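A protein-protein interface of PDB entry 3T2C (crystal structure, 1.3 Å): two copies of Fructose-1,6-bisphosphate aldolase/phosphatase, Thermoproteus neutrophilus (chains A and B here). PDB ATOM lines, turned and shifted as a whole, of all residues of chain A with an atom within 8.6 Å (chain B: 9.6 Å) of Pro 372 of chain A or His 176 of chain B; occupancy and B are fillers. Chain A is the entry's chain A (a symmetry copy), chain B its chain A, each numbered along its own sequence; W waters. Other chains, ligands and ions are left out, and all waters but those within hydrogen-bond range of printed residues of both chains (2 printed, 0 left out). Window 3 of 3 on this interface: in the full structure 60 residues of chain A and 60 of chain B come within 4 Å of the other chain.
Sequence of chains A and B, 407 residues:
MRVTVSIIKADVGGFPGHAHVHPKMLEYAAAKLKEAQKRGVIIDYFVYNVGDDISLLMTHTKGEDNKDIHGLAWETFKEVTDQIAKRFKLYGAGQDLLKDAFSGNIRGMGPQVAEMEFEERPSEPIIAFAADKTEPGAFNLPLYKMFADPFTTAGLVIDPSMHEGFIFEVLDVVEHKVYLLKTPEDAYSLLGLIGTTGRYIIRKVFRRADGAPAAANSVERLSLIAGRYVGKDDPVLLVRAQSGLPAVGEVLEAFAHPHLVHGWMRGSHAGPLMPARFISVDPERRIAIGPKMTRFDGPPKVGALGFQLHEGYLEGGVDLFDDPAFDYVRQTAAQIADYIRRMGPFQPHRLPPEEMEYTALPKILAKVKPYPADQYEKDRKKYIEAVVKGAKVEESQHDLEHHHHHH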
ATOM      1  N   LYS A 369      -2.606  15.778  -8.940  1.00  0.00           N
ATOM      2  CA  LYS A 369      -1.913  17.129  -9.011  1.00  0.00           C
ATOM      3  C   LYS A 369      -0.471  17.270  -8.609  1.00  0.00           C
ATOM      4  O   LYS A 369      -0.143  17.307  -7.385  1.00  0.00           O
ATOM      5  CB  LYS A 369      -2.659  18.128  -8.084  1.00  0.00           C
ATOM      6  N   PRO A 370       0.461  17.295  -9.578  1.00  0.00           N
ATOM      7  CA  PRO A 370       1.919  17.411  -9.261  1.00  0.00           C
ATOM      8  C   PRO A 370       2.400  18.838  -9.079  1.00  0.00           C
ATOM      9  O   PRO A 370       1.920  19.752  -9.802  1.00  0.00           O
ATOM     10  CB  PRO A 370       2.575  16.962 -10.597  1.00  0.00           C
ATOM     11  CG  PRO A 370       1.462  16.386 -11.355  1.00  0.00           C
ATOM     12  CD  PRO A 370       0.292  17.276 -11.031  1.00  0.00           C
ATOM     13  N   TYR A 371       3.378  19.043  -8.220  1.00  0.00           N
ATOM     14  CA  TYR A 371       4.149  20.266  -8.143  1.00  0.00           C
ATOM     15  C   TYR A 371       5.574  20.033  -8.599  1.00  0.00           C
ATOM     16  O   TYR A 371       6.205  19.073  -8.255  1.00  0.00           O
ATOM     17  CB  TYR A 371       4.237  20.721  -6.706  1.00  0.00           C
ATOM     18  CG  TYR A 371       2.916  20.904  -6.035  1.00  0.00           C
ATOM     19  CD1 TYR A 371       2.193  22.055  -6.234  1.00  0.00           C
ATOM     20  CD2 TYR A 371       2.400  19.978  -5.197  1.00  0.00           C
ATOM     21  CE1 TYR A 371       0.981  22.246  -5.638  1.00  0.00           C
ATOM     22  CE2 TYR A 371       1.191  20.157  -4.576  1.00  0.00           C
ATOM     23  CZ  TYR A 371       0.478  21.294  -4.789  1.00  0.00           C
ATOM     24  OH  TYR A 371      -0.718  21.437  -4.142  1.00  0.00           O
ATOM     25  N   PRO A 372       6.129  20.949  -9.404  1.00  0.00           N
ATOM     26  CA  PRO A 372       7.568  20.872  -9.739  1.00  0.00           C
ATOM     27  C   PRO A 372       8.420  20.849  -8.493  1.00  0.00           C
ATOM     28  O   PRO A 372       8.222  21.655  -7.585  1.00  0.00           O
ATOM     29  CB  PRO A 372       7.812  22.145 -10.542  1.00  0.00           C
ATOM     30  CG  PRO A 372       6.479  22.454 -11.113  1.00  0.00           C
ATOM     31  CD  PRO A 372       5.488  22.118 -10.063  1.00  0.00           C
ATOM     32  N   ALA A 373       9.344  19.915  -8.393  1.00  0.00           N
ATOM     33  CA  ALA A 373      10.002  19.706  -7.116  1.00  0.00           C
ATOM     34  C   ALA A 373      10.794  20.890  -6.570  1.00  0.00           C
ATOM     35  O   ALA A 373      10.857  21.111  -5.347  1.00  0.00           O
ATOM     36  CB  ALA A 373      10.889  18.458  -7.135  1.00  0.00           C
ATOM     37  N   ASP A 374      11.454  21.629  -7.447  1.00  0.00           N
ATOM     38  CA  ASP A 374      12.321  22.745  -6.961  1.00  0.00           C
ATOM     39  C   ASP A 374      11.456  23.857  -6.356  1.00  0.00           C
ATOM     40  O   ASP A 374      11.704  24.368  -5.246  1.00  0.00           O
ATOM     41  CB  ASP A 374      13.289  23.206  -8.050  1.00  0.00           C
ATOM     42  CG  ASP A 374      14.315  22.162  -8.416  1.00  0.00           C
ATOM     43  OD1 ASP A 374      14.634  21.240  -7.591  1.00  0.00           O
ATOM     44  OD2 ASP A 374      14.798  22.255  -9.583  1.00  0.00           O
ATOM     45  N   GLN A 375      10.370  24.130  -6.998  1.00  0.00           N
ATOM     46  CA  GLN A 375       9.478  25.133  -6.525  1.00  0.00           C
ATOM     47  C   GLN A 375       8.787  24.671  -5.252  1.00  0.00           C
ATOM     48  O   GLN A 375       8.566  25.449  -4.298  1.00  0.00           O
ATOM     49  CB  GLN A 375       8.462  25.441  -7.647  1.00  0.00           C
ATOM     50  CG  GLN A 375       9.024  25.582  -9.181  1.00  0.00           C
ATOM     51  CD  GLN A 375      10.549  25.098  -9.536  1.00  0.00           C
ATOM     52  OE1 GLN A 375      10.834  23.865  -9.753  1.00  0.00           O
ATOM     53  NE2 GLN A 375      11.497  26.130  -9.679  1.00  0.00           N
ATOM     54  N   TYR A 376       8.418  23.397  -5.232  1.00  0.00           N
ATOM     55  CA  TYR A 376       7.736  22.880  -4.034  1.00  0.00           C
ATOM     56  C   TYR A 376       8.583  23.071  -2.795  1.00  0.00           C
ATOM     57  O   TYR A 376       8.035  23.378  -1.749  1.00  0.00           O
ATOM     58  CB  TYR A 376       7.519  21.401  -4.232  1.00  0.00           C
ATOM     59  CG  TYR A 376       6.920  20.731  -2.988  1.00  0.00           C
ATOM     60  CD1 TYR A 376       5.555  20.744  -2.715  1.00  0.00           C
ATOM     61  CD2 TYR A 376       7.750  20.123  -2.047  1.00  0.00           C
ATOM     62  CE1 TYR A 376       5.025  20.201  -1.569  1.00  0.00           C
ATOM     63  CE2 TYR A 376       7.198  19.592  -0.872  1.00  0.00           C
ATOM     64  CZ  TYR A 376       5.872  19.637  -0.644  1.00  0.00           C
ATOM     65  OH  TYR A 376       5.307  19.101   0.484  1.00  0.00           O
ATOM     66  N   GLU A 377       9.887  22.898  -2.880  1.00  0.00           N
ATOM     67  CA  GLU A 377      10.686  23.080  -1.693  1.00  0.00           C
ATOM     68  C   GLU A 377      10.521  24.456  -1.029  1.00  0.00           C
ATOM     69  O   GLU A 377      10.529  24.580   0.206  1.00  0.00           O
ATOM     70  CB  GLU A 377      12.159  23.131  -2.056  1.00  0.00           C
ATOM     71  CG  GLU A 377      12.767  21.890  -2.321  1.00  0.00           C
ATOM     72  CD  GLU A 377      12.796  20.983  -1.110  1.00  0.00           C
ATOM     73  OE1 GLU A 377      13.122  21.395   0.062  1.00  0.00           O
ATOM     74  OE2 GLU A 377      12.505  19.809  -1.357  1.00  0.00           O
ATOM     75  N   LYS A 378      10.403  25.494  -1.873  1.00  0.00           N
ATOM     76  CA  LYS A 378      10.182  26.866  -1.348  1.00  0.00           C
ATOM     77  C   LYS A 378       8.805  26.999  -0.663  1.00  0.00           C
ATOM     78  O   LYS A 378       8.623  27.781   0.266  1.00  0.00           O
ATOM     79  CB  LYS A 378      10.292  27.934  -2.497  1.00  0.00           C
ATOM     80  CG  LYS A 378      11.600  27.863  -3.263  1.00  0.00           C
ATOM     81  CD  LYS A 378      11.764  29.040  -4.301  1.00  0.00           C
ATOM     82  CE  LYS A 378      11.373  28.659  -5.794  1.00  0.00           C
ATOM     83  NZ  LYS A 378      12.488  28.096  -6.675  1.00  0.00           N
ATOM     84  N   ASP A 379       7.815  26.331  -1.210  1.00  0.00           N
ATOM     85  CA  ASP A 379       6.392  26.512  -0.916  1.00  0.00           C
ATOM     86  C   ASP A 379       5.842  25.483   0.079  1.00  0.00           C
ATOM     87  O   ASP A 379       4.633  25.497   0.397  1.00  0.00           O
ATOM     88  CB  ASP A 379       5.532  26.494  -2.213  1.00  0.00           C
ATOM     89  CG  ASP A 379       5.849  27.690  -3.150  1.00  0.00           C
ATOM     90  OD1 ASP A 379       6.171  28.806  -2.603  1.00  0.00           O
ATOM     91  OD2 ASP A 379       5.767  27.506  -4.440  1.00  0.00           O
ATOM     92  N   TYR A 383       1.969  24.999   1.407  1.00  0.00           N
ATOM     93  CA  TYR A 383       1.081  23.907   0.964  1.00  0.00           C
ATOM     94  C   TYR A 383       0.587  23.068   2.088  1.00  0.00           C
ATOM     95  O   TYR A 383      -0.622  22.680   2.113  1.00  0.00           O
ATOM     96  CB  TYR A 383       1.748  23.027   0.002  1.00  0.00           C
ATOM     97  CG  TYR A 383       1.996  23.652  -1.313  1.00  0.00           C
ATOM     98  CD1 TYR A 383       1.106  24.533  -1.888  1.00  0.00           C
ATOM     99  CD2 TYR A 383       3.182  23.457  -1.944  1.00  0.00           C
ATOM    100  CE1 TYR A 383       1.397  25.132  -3.143  1.00  0.00           C
ATOM    101  CE2 TYR A 383       3.480  24.018  -3.137  1.00  0.00           C
ATOM    102  CZ  TYR A 383       2.612  24.870  -3.756  1.00  0.00           C
ATOM    103  OH  TYR A 383       2.962  25.406  -4.996  1.00  0.00           O
ATOM    104  N   GLU B 169       4.025  13.381   1.451  1.00  0.00           N
ATOM    105  CA  GLU B 169       4.778  14.068   0.424  1.00  0.00           C
ATOM    106  C   GLU B 169       5.574  13.004  -0.339  1.00  0.00           C
ATOM    107  O   GLU B 169       6.491  12.407   0.173  1.00  0.00           O
ATOM    108  CB  GLU B 169       5.697  15.061   1.061  1.00  0.00           C
ATOM    109  CG  GLU B 169       6.636  15.779   0.093  1.00  0.00           C
ATOM    110  CD  GLU B 169       7.586  16.713   0.792  1.00  0.00           C
ATOM    111  OE1 GLU B 169       8.812  16.607   0.498  1.00  0.00           O
ATOM    112  OE2 GLU B 169       7.126  17.528   1.661  1.00  0.00           O
ATOM    113  N   VAL B 170       5.136  12.802  -1.588  1.00  0.00           N
ATOM    114  CA  VAL B 170       5.627  11.742  -2.457  1.00  0.00           C
ATOM    115  C   VAL B 170       6.432  12.390  -3.553  1.00  0.00           C
ATOM    116  O   VAL B 170       5.916  13.281  -4.287  1.00  0.00           O
ATOM    117  CB  VAL B 170       4.484  10.887  -3.044  1.00  0.00           C
ATOM    118  CG1 VAL B 170       5.000   9.878  -4.057  1.00  0.00           C
ATOM    119  CG2 VAL B 170       3.653  10.233  -1.936  1.00  0.00           C
ATOM    120  N   LEU B 171       7.678  11.941  -3.750  1.00  0.00           N
ATOM    121  CA  LEU B 171       8.571  12.436  -4.760  1.00  0.00           C
ATOM    122  C   LEU B 171       8.598  11.456  -5.943  1.00  0.00           C
ATOM    123  O   LEU B 171       8.976  10.286  -5.762  1.00  0.00           O
ATOM    124  CB  LEU B 171       9.978  12.664  -4.202  1.00  0.00           C
ATOM    125  CG  LEU B 171      11.050  13.215  -5.189  1.00  0.00           C
ATOM    126  CD1 LEU B 171      10.669  14.619  -5.698  1.00  0.00           C
ATOM    127  CD2 LEU B 171      12.372  13.230  -4.461  1.00  0.00           C
ATOM    128  N   ASP B 172       8.301  11.970  -7.120  1.00  0.00           N
ATOM    129  CA  ASP B 172       8.586  11.274  -8.389  1.00  0.00           C
ATOM    130  C   ASP B 172      10.043  11.605  -8.767  1.00  0.00           C
ATOM    131  O   ASP B 172      10.362  12.741  -9.145  1.00  0.00           O
ATOM    132  CB  ASP B 172       7.632  11.796  -9.455  1.00  0.00           C
ATOM    133  CG  ASP B 172       7.909  11.294 -10.857  1.00  0.00           C
ATOM    134  OD1 ASP B 172       8.948  10.644 -11.113  1.00  0.00           O
ATOM    135  OD2 ASP B 172       7.033  11.598 -11.723  1.00  0.00           O
ATOM    136  N   VAL B 173      10.923  10.627  -8.519  1.00  0.00           N
ATOM    137  CA  VAL B 173      12.357  10.827  -8.679  1.00  0.00           C
ATOM    138  C   VAL B 173      12.781  10.855 -10.137  1.00  0.00           C
ATOM    139  O   VAL B 173      13.921  11.245 -10.441  1.00  0.00           O
ATOM    140  CB  VAL B 173      13.155   9.760  -7.888  1.00  0.00           C
ATOM    141  CG1 VAL B 173      12.846   9.947  -6.399  1.00  0.00           C
ATOM    142  CG2 VAL B 173      12.886   8.306  -8.331  1.00  0.00           C
ATOM    143  N   VAL B 174      11.907  10.474 -11.055  1.00  0.00           N
ATOM    144  CA  VAL B 174      12.248  10.450 -12.452  1.00  0.00           C
ATOM    145  C   VAL B 174      11.949  11.829 -13.066  1.00  0.00           C
ATOM    146  O   VAL B 174      12.821  12.390 -13.715  1.00  0.00           O
ATOM    147  CB  VAL B 174      11.501   9.332 -13.183  1.00  0.00           C
ATOM    148  CG1 VAL B 174      11.689   9.475 -14.680  1.00  0.00           C
ATOM    149  CG2 VAL B 174      11.933   7.925 -12.711  1.00  0.00           C
ATOM    150  N   GLU B 175      10.735  12.330 -12.909  1.00  0.00           N
ATOM    151  CA  GLU B 175      10.322  13.618 -13.443  1.00  0.00           C
ATOM    152  C   GLU B 175      10.464  14.772 -12.501  1.00  0.00           C
ATOM    153  O   GLU B 175      10.212  15.935 -12.894  1.00  0.00           O
ATOM    154  CB  GLU B 175       8.900  13.538 -13.980  1.00  0.00           C
ATOM    155  CG  GLU B 175       8.779  12.605 -15.172  1.00  0.00           C
ATOM    156  CD  GLU B 175       7.344  12.599 -15.809  1.00  0.00           C
ATOM    157  OE1 GLU B 175       6.376  13.288 -15.299  1.00  0.00           O
ATOM    158  OE2 GLU B 175       7.175  11.829 -16.775  1.00  0.00           O
ATOM    159  N   HIS B 176      10.904  14.543 -11.262  1.00  0.00           N
ATOM    160  CA  HIS B 176      11.195  15.618 -10.313  1.00  0.00           C
ATOM    161  C   HIS B 176       9.907  16.399 -10.033  1.00  0.00           C
ATOM    162  O   HIS B 176       9.844  17.641 -10.185  1.00  0.00           O
ATOM    163  CB  HIS B 176      12.350  16.545 -10.718  1.00  0.00           C
ATOM    164  CG  HIS B 176      13.475  15.848 -11.359  1.00  0.00           C
ATOM    165  ND1 HIS B 176      14.313  14.981 -10.713  1.00  0.00           N
ATOM    166  CD2 HIS B 176      13.917  15.906 -12.635  1.00  0.00           C
ATOM    167  CE1 HIS B 176      15.255  14.555 -11.551  1.00  0.00           C
ATOM    168  NE2 HIS B 176      15.022  15.092 -12.728  1.00  0.00           N
ATOM    169  N   LYS B 177       8.885  15.700  -9.548  1.00  0.00           N
ATOM    170  CA  LYS B 177       7.573  16.246  -9.245  1.00  0.00           C
ATOM    171  C   LYS B 177       7.174  15.761  -7.861  1.00  0.00           C
ATOM    172  O   LYS B 177       7.527  14.632  -7.494  1.00  0.00           O
ATOM    173  CB  LYS B 177       6.549  15.781 -10.299  1.00  0.00           C
ATOM    174  CG  LYS B 177       6.860  16.309 -11.662  1.00  0.00           C
ATOM    175  CD  LYS B 177       5.903  15.845 -12.731  1.00  0.00           C
ATOM    176  CE  LYS B 177       6.259  16.570 -14.049  1.00  0.00           C
ATOM    177  NZ  LYS B 177       5.575  15.902 -15.200  1.00  0.00           N
ATOM    178  N   VAL B 178       6.441  16.544  -7.136  1.00  0.00           N
ATOM    179  CA  VAL B 178       5.998  16.216  -5.781  1.00  0.00           C
ATOM    180  C   VAL B 178       4.472  16.156  -5.776  1.00  0.00           C
ATOM    181  O   VAL B 178       3.779  16.997  -6.342  1.00  0.00           O
ATOM    182  CB  VAL B 178       6.499  17.238  -4.764  1.00  0.00           C
ATOM    183  CG1 VAL B 178       5.858  16.993  -3.365  1.00  0.00           C
ATOM    184  CG2 VAL B 178       8.010  17.287  -4.725  1.00  0.00           C
ATOM    185  N   TYR B 179       3.948  15.137  -5.124  1.00  0.00           N
ATOM    186  CA  TYR B 179       2.539  14.917  -4.889  1.00  0.00           C
ATOM    187  C   TYR B 179       2.321  15.059  -3.389  1.00  0.00           C
ATOM    188  O   TYR B 179       3.058  14.496  -2.600  1.00  0.00           O
ATOM    189  CB  TYR B 179       2.021  13.546  -5.421  1.00  0.00           C
ATOM    190  CG  TYR B 179       2.290  13.426  -6.925  1.00  0.00           C
ATOM    191  CD1 TYR B 179       3.484  12.986  -7.435  1.00  0.00           C
ATOM    192  CD2 TYR B 179       1.327  13.863  -7.831  1.00  0.00           C
ATOM    193  CE1 TYR B 179       3.749  13.012  -8.820  1.00  0.00           C
ATOM    194  CE2 TYR B 179       1.590  13.897  -9.215  1.00  0.00           C
ATOM    195  CZ  TYR B 179       2.820  13.532  -9.698  1.00  0.00           C
ATOM    196  OH  TYR B 179       3.044  13.586 -11.106  1.00  0.00           O
ATOM    197  N   ARG B 199      10.079   4.624  -8.348  1.00  0.00           N
ATOM    198  CA  ARG B 199       9.771   5.915  -8.930  1.00  0.00           C
ATOM    199  C   ARG B 199       9.126   6.891  -8.003  1.00  0.00           C
ATOM    200  O   ARG B 199       9.534   8.070  -7.958  1.00  0.00           O
ATOM    201  CB  ARG B 199       8.914   5.799 -10.190  1.00  0.00           C
ATOM    202  CG  ARG B 199       8.668   7.147 -10.786  1.00  0.00           C
ATOM    203  CD  ARG B 199       8.087   7.040 -12.143  1.00  0.00           C
ATOM    204  NE  ARG B 199       7.810   8.376 -12.640  1.00  0.00           N
ATOM    205  CZ  ARG B 199       7.268   8.658 -13.794  1.00  0.00           C
ATOM    206  NH1 ARG B 199       7.028   7.683 -14.634  1.00  0.00           N
ATOM    207  NH2 ARG B 199       6.994   9.886 -14.073  1.00  0.00           N
ATOM    208  N   TYR B 200       8.101   6.477  -7.271  1.00  0.00           N
ATOM    209  CA  TYR B 200       7.329   7.338  -6.409  1.00  0.00           C
ATOM    210  C   TYR B 200       7.619   6.955  -4.966  1.00  0.00           C
ATOM    211  O   TYR B 200       7.158   5.904  -4.496  1.00  0.00           O
ATOM    212  CB  TYR B 200       5.830   7.240  -6.683  1.00  0.00           C
ATOM    213  CG  TYR B 200       5.408   7.627  -8.048  1.00  0.00           C
ATOM    214  CD1 TYR B 200       5.291   8.917  -8.428  1.00  0.00           C
ATOM    215  CD2 TYR B 200       5.149   6.690  -9.026  1.00  0.00           C
ATOM    216  CE1 TYR B 200       4.909   9.268  -9.674  1.00  0.00           C
ATOM    217  CE2 TYR B 200       4.712   7.026 -10.299  1.00  0.00           C
ATOM    218  CZ  TYR B 200       4.648   8.370 -10.597  1.00  0.00           C
ATOM    219  OH  TYR B 200       4.182   8.786 -11.877  1.00  0.00           O
ATOM    220  N   ARG B 203       8.674  10.728   0.807  1.00  0.00           N
ATOM    221  CA  ARG B 203       9.801  11.505   1.328  1.00  0.00           C
ATOM    222  C   ARG B 203       9.528  12.053   2.710  1.00  0.00           C
ATOM    223  O   ARG B 203      10.412  12.035   3.573  1.00  0.00           O
ATOM    224  CB  ARG B 203      10.150  12.659   0.342  1.00  0.00           C
ATOM    225  CG  ARG B 203      11.426  13.372   0.786  1.00  0.00           C
ATOM    226  CD  ARG B 203      11.978  14.340  -0.283  1.00  0.00           C
ATOM    227  NE  ARG B 203      11.012  15.315  -0.742  1.00  0.00           N
ATOM    228  CZ  ARG B 203      11.200  16.220  -1.698  1.00  0.00           C
ATOM    229  NH1 ARG B 203      12.302  16.239  -2.447  1.00  0.00           N
ATOM    230  NH2 ARG B 203      10.281  16.951  -1.954  1.00  0.00           N
ATOM    231  N   VAL B 219      15.606  10.191   0.022  1.00  0.00           N
ATOM    232  CA  VAL B 219      15.370   9.715  -1.360  1.00  0.00           C
ATOM    233  C   VAL B 219      16.397   9.757  -2.491  1.00  0.00           C
ATOM    234  O   VAL B 219      16.035   9.955  -3.671  1.00  0.00           O
ATOM    235  CB  VAL B 219      14.058  10.263  -1.858  1.00  0.00           C
ATOM    236  CG1 VAL B 219      13.653   9.172  -3.054  1.00  0.00           C
ATOM    237  CG2 VAL B 219      12.899  10.529  -0.920  1.00  0.00           C
ATOM    238  N   GLU B 220      17.657   9.567  -2.207  1.00  0.00           N
ATOM    239  CA  GLU B 220      18.665   9.700  -3.220  1.00  0.00           C
ATOM    240  C   GLU B 220      18.681   8.351  -3.975  1.00  0.00           C
ATOM    241  O   GLU B 220      18.970   7.308  -3.407  1.00  0.00           O
ATOM    242  CB  GLU B 220      20.032  10.094  -2.602  1.00  0.00           C
ATOM    243  CG  GLU B 220      19.945  11.293  -1.665  1.00  0.00           C
ATOM    244  CD  GLU B 220      19.394  12.522  -2.352  1.00  0.00           C
ATOM    245  OE1 GLU B 220      18.455  13.141  -1.828  1.00  0.00           O
ATOM    246  OE2 GLU B 220      19.952  12.897  -3.358  1.00  0.00           O
ATOM    247  N   ARG B 221      18.686   8.454  -5.249  1.00  0.00           N
ATOM    248  CA  ARG B 221      18.843   7.307  -6.171  1.00  0.00           C
ATOM    249  C   ARG B 221      20.183   7.365  -6.902  1.00  0.00           C
ATOM    250  O   ARG B 221      20.414   8.191  -7.793  1.00  0.00           O
ATOM    251  CB  ARG B 221      17.701   7.270  -7.169  1.00  0.00           C
ATOM    252  CG  ARG B 221      16.344   7.156  -6.504  1.00  0.00           C
ATOM    253  CD  ARG B 221      16.341   5.766  -5.917  1.00  0.00           C
ATOM    254  NE  ARG B 221      15.586   4.993  -6.817  1.00  0.00           N
ATOM    255  CZ  ARG B 221      15.772   3.800  -7.447  1.00  0.00           C
ATOM    256  NH1 ARG B 221      14.827   3.470  -8.316  1.00  0.00           N
ATOM    257  NH2 ARG B 221      16.646   2.830  -7.176  1.00  0.00           N
ATOM    258  N   LEU B 224      20.459   7.326 -10.612  1.00  0.00           N
ATOM    259  CA  LEU B 224      20.057   8.496 -11.366  1.00  0.00           C
ATOM    260  C   LEU B 224      21.144   9.564 -11.249  1.00  0.00           C
ATOM    261  O   LEU B 224      21.461  10.272 -12.191  1.00  0.00           O
ATOM    262  CB  LEU B 224      18.694   9.020 -10.823  1.00  0.00           C
ATOM    263  CG  LEU B 224      17.469   8.115 -11.103  1.00  0.00           C
ATOM    264  CD1 LEU B 224      16.233   8.776 -10.666  1.00  0.00           C
ATOM    265  CD2 LEU B 224      17.418   7.765 -12.613  1.00  0.00           C
ATOM    266  N   ILE B 225      21.797   9.639 -10.072  1.00  0.00           N
ATOM    267  CA  ILE B 225      22.966  10.461  -9.885  1.00  0.00           C
ATOM    268  C   ILE B 225      24.107  10.065 -10.855  1.00  0.00           C
ATOM    269  O   ILE B 225      24.626  10.932 -11.546  1.00  0.00           O
ATOM    270  CB  ILE B 225      23.479  10.494  -8.421  1.00  0.00           C
ATOM    271  CG1 ILE B 225      22.425  11.125  -7.487  1.00  0.00           C
ATOM    272  CG2 ILE B 225      24.752  11.311  -8.322  1.00  0.00           C
ATOM    273  CD1 ILE B 225      22.734  10.988  -5.986  1.00  0.00           C
HETATM  274  O   HOH W   1      10.013  19.664 -11.740  1.00  0.00           O
HETATM  275  O   HOH W   2      11.303  19.007  -3.510  1.00  0.00           O
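O of Tyr 371 of chain A sits at hydrogen-bond distance from N of Val 178 of chain B.
The backbone NH (N) of Ala 373 of chain A is in hydrogen-bond range of the backbone carbonyl oxygen (O) of His 176 of chain B (2.9 Å).
The guanidinium group of Arg 203 of chain B is in salt-bridge range of the side-chain carboxylate of Glu 377 of chain A (3.7 Å).
OE2 of Glu 169 of chain B is in hydrogen-bond range of OH of Tyr 376 of chain A (2.7 Å).
OE1 of Glu 169 of chain B lies within salt-bridge range of NE of Arg 203 of chain B.
The backbone carbonyl oxygen (O) of Val 170 of chain B lies within hydrogen-bond range of the backbone NH (N) of Tyr 179 of chain B (2.8 Å).
O of Lys 177 of chain B lies within hydrogen-bond range of N of Asp 172 of chain B, at 2.8 Å.
OE1 of Glu 175 of chain B lies within salt-bridge range of NZ of Lys 177 of chain B, at 2.7 Å.
Among the printed residues, pairs that only touch across the chains: Pro 370 of chain A with Tyr 179 of chain B (3.2 Å), Tyr 371 of chain A with Lys 177 of chain B (3.3 Å), Pro 370 of chain A with Val 178 of chain B (3.5 Å), Tyr 376 of chain A with Val 178 of chain B (3.8 Å), Lys 369 of chain A with Tyr 179 of chain B (3.8 Å), Pro 372 of chain A with His 176 of chain B (3.9 Å) and Ala 373 of chain A with Val 178 of chain B (3.9 Å).
Pro 372 of chain A touches just one residue of chain B: His 176 (3.9 Å).
No residue of chain B comes within 4 Å of Gln 375 of chain A.
Printed residues of chain A within 4 Å of Tyr 179 of chain B: Lys 369 and Pro 370.
Of the printed residues of chain A, Lys 177 of chain B touches Tyr 371.
Printed residues of chain A that touch a printed residue of chain B: Lys 369, Pro 370, Tyr 371, Pro 372, Ala 373, Tyr 376 and Glu 377.
Hydrophobic or aromatic side chains of chain A that line the printed part of chain B: Pro 370, Tyr 371, Ala 373 and Tyr 376.
Among the printed residues, Asp or Glu carboxylates within 4 Å of a Lys or Arg side-chain nitrogen of the other chain: Glu 377 of chain A with Arg 203 of chain B.
No position is printed for both chains.
Of the 11 pairs that touch across the chains among the printed residues, none has its exchanged pair printed and touching as well.
Water W1 lies within hydrogen-bond range of O of His 176 of chain B and N of Ala 373 of chain A.
Water W2 lies within hydrogen-bond range of the side-chain carboxylate (OE2) of Glu 377 of chain A (2.6 Å), the guanidinium group (NH2) of Arg 203 of chain B (2.8 Å) and the backbone carbonyl oxygen (O) of Ala 373 of chain A (2.8 Å).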
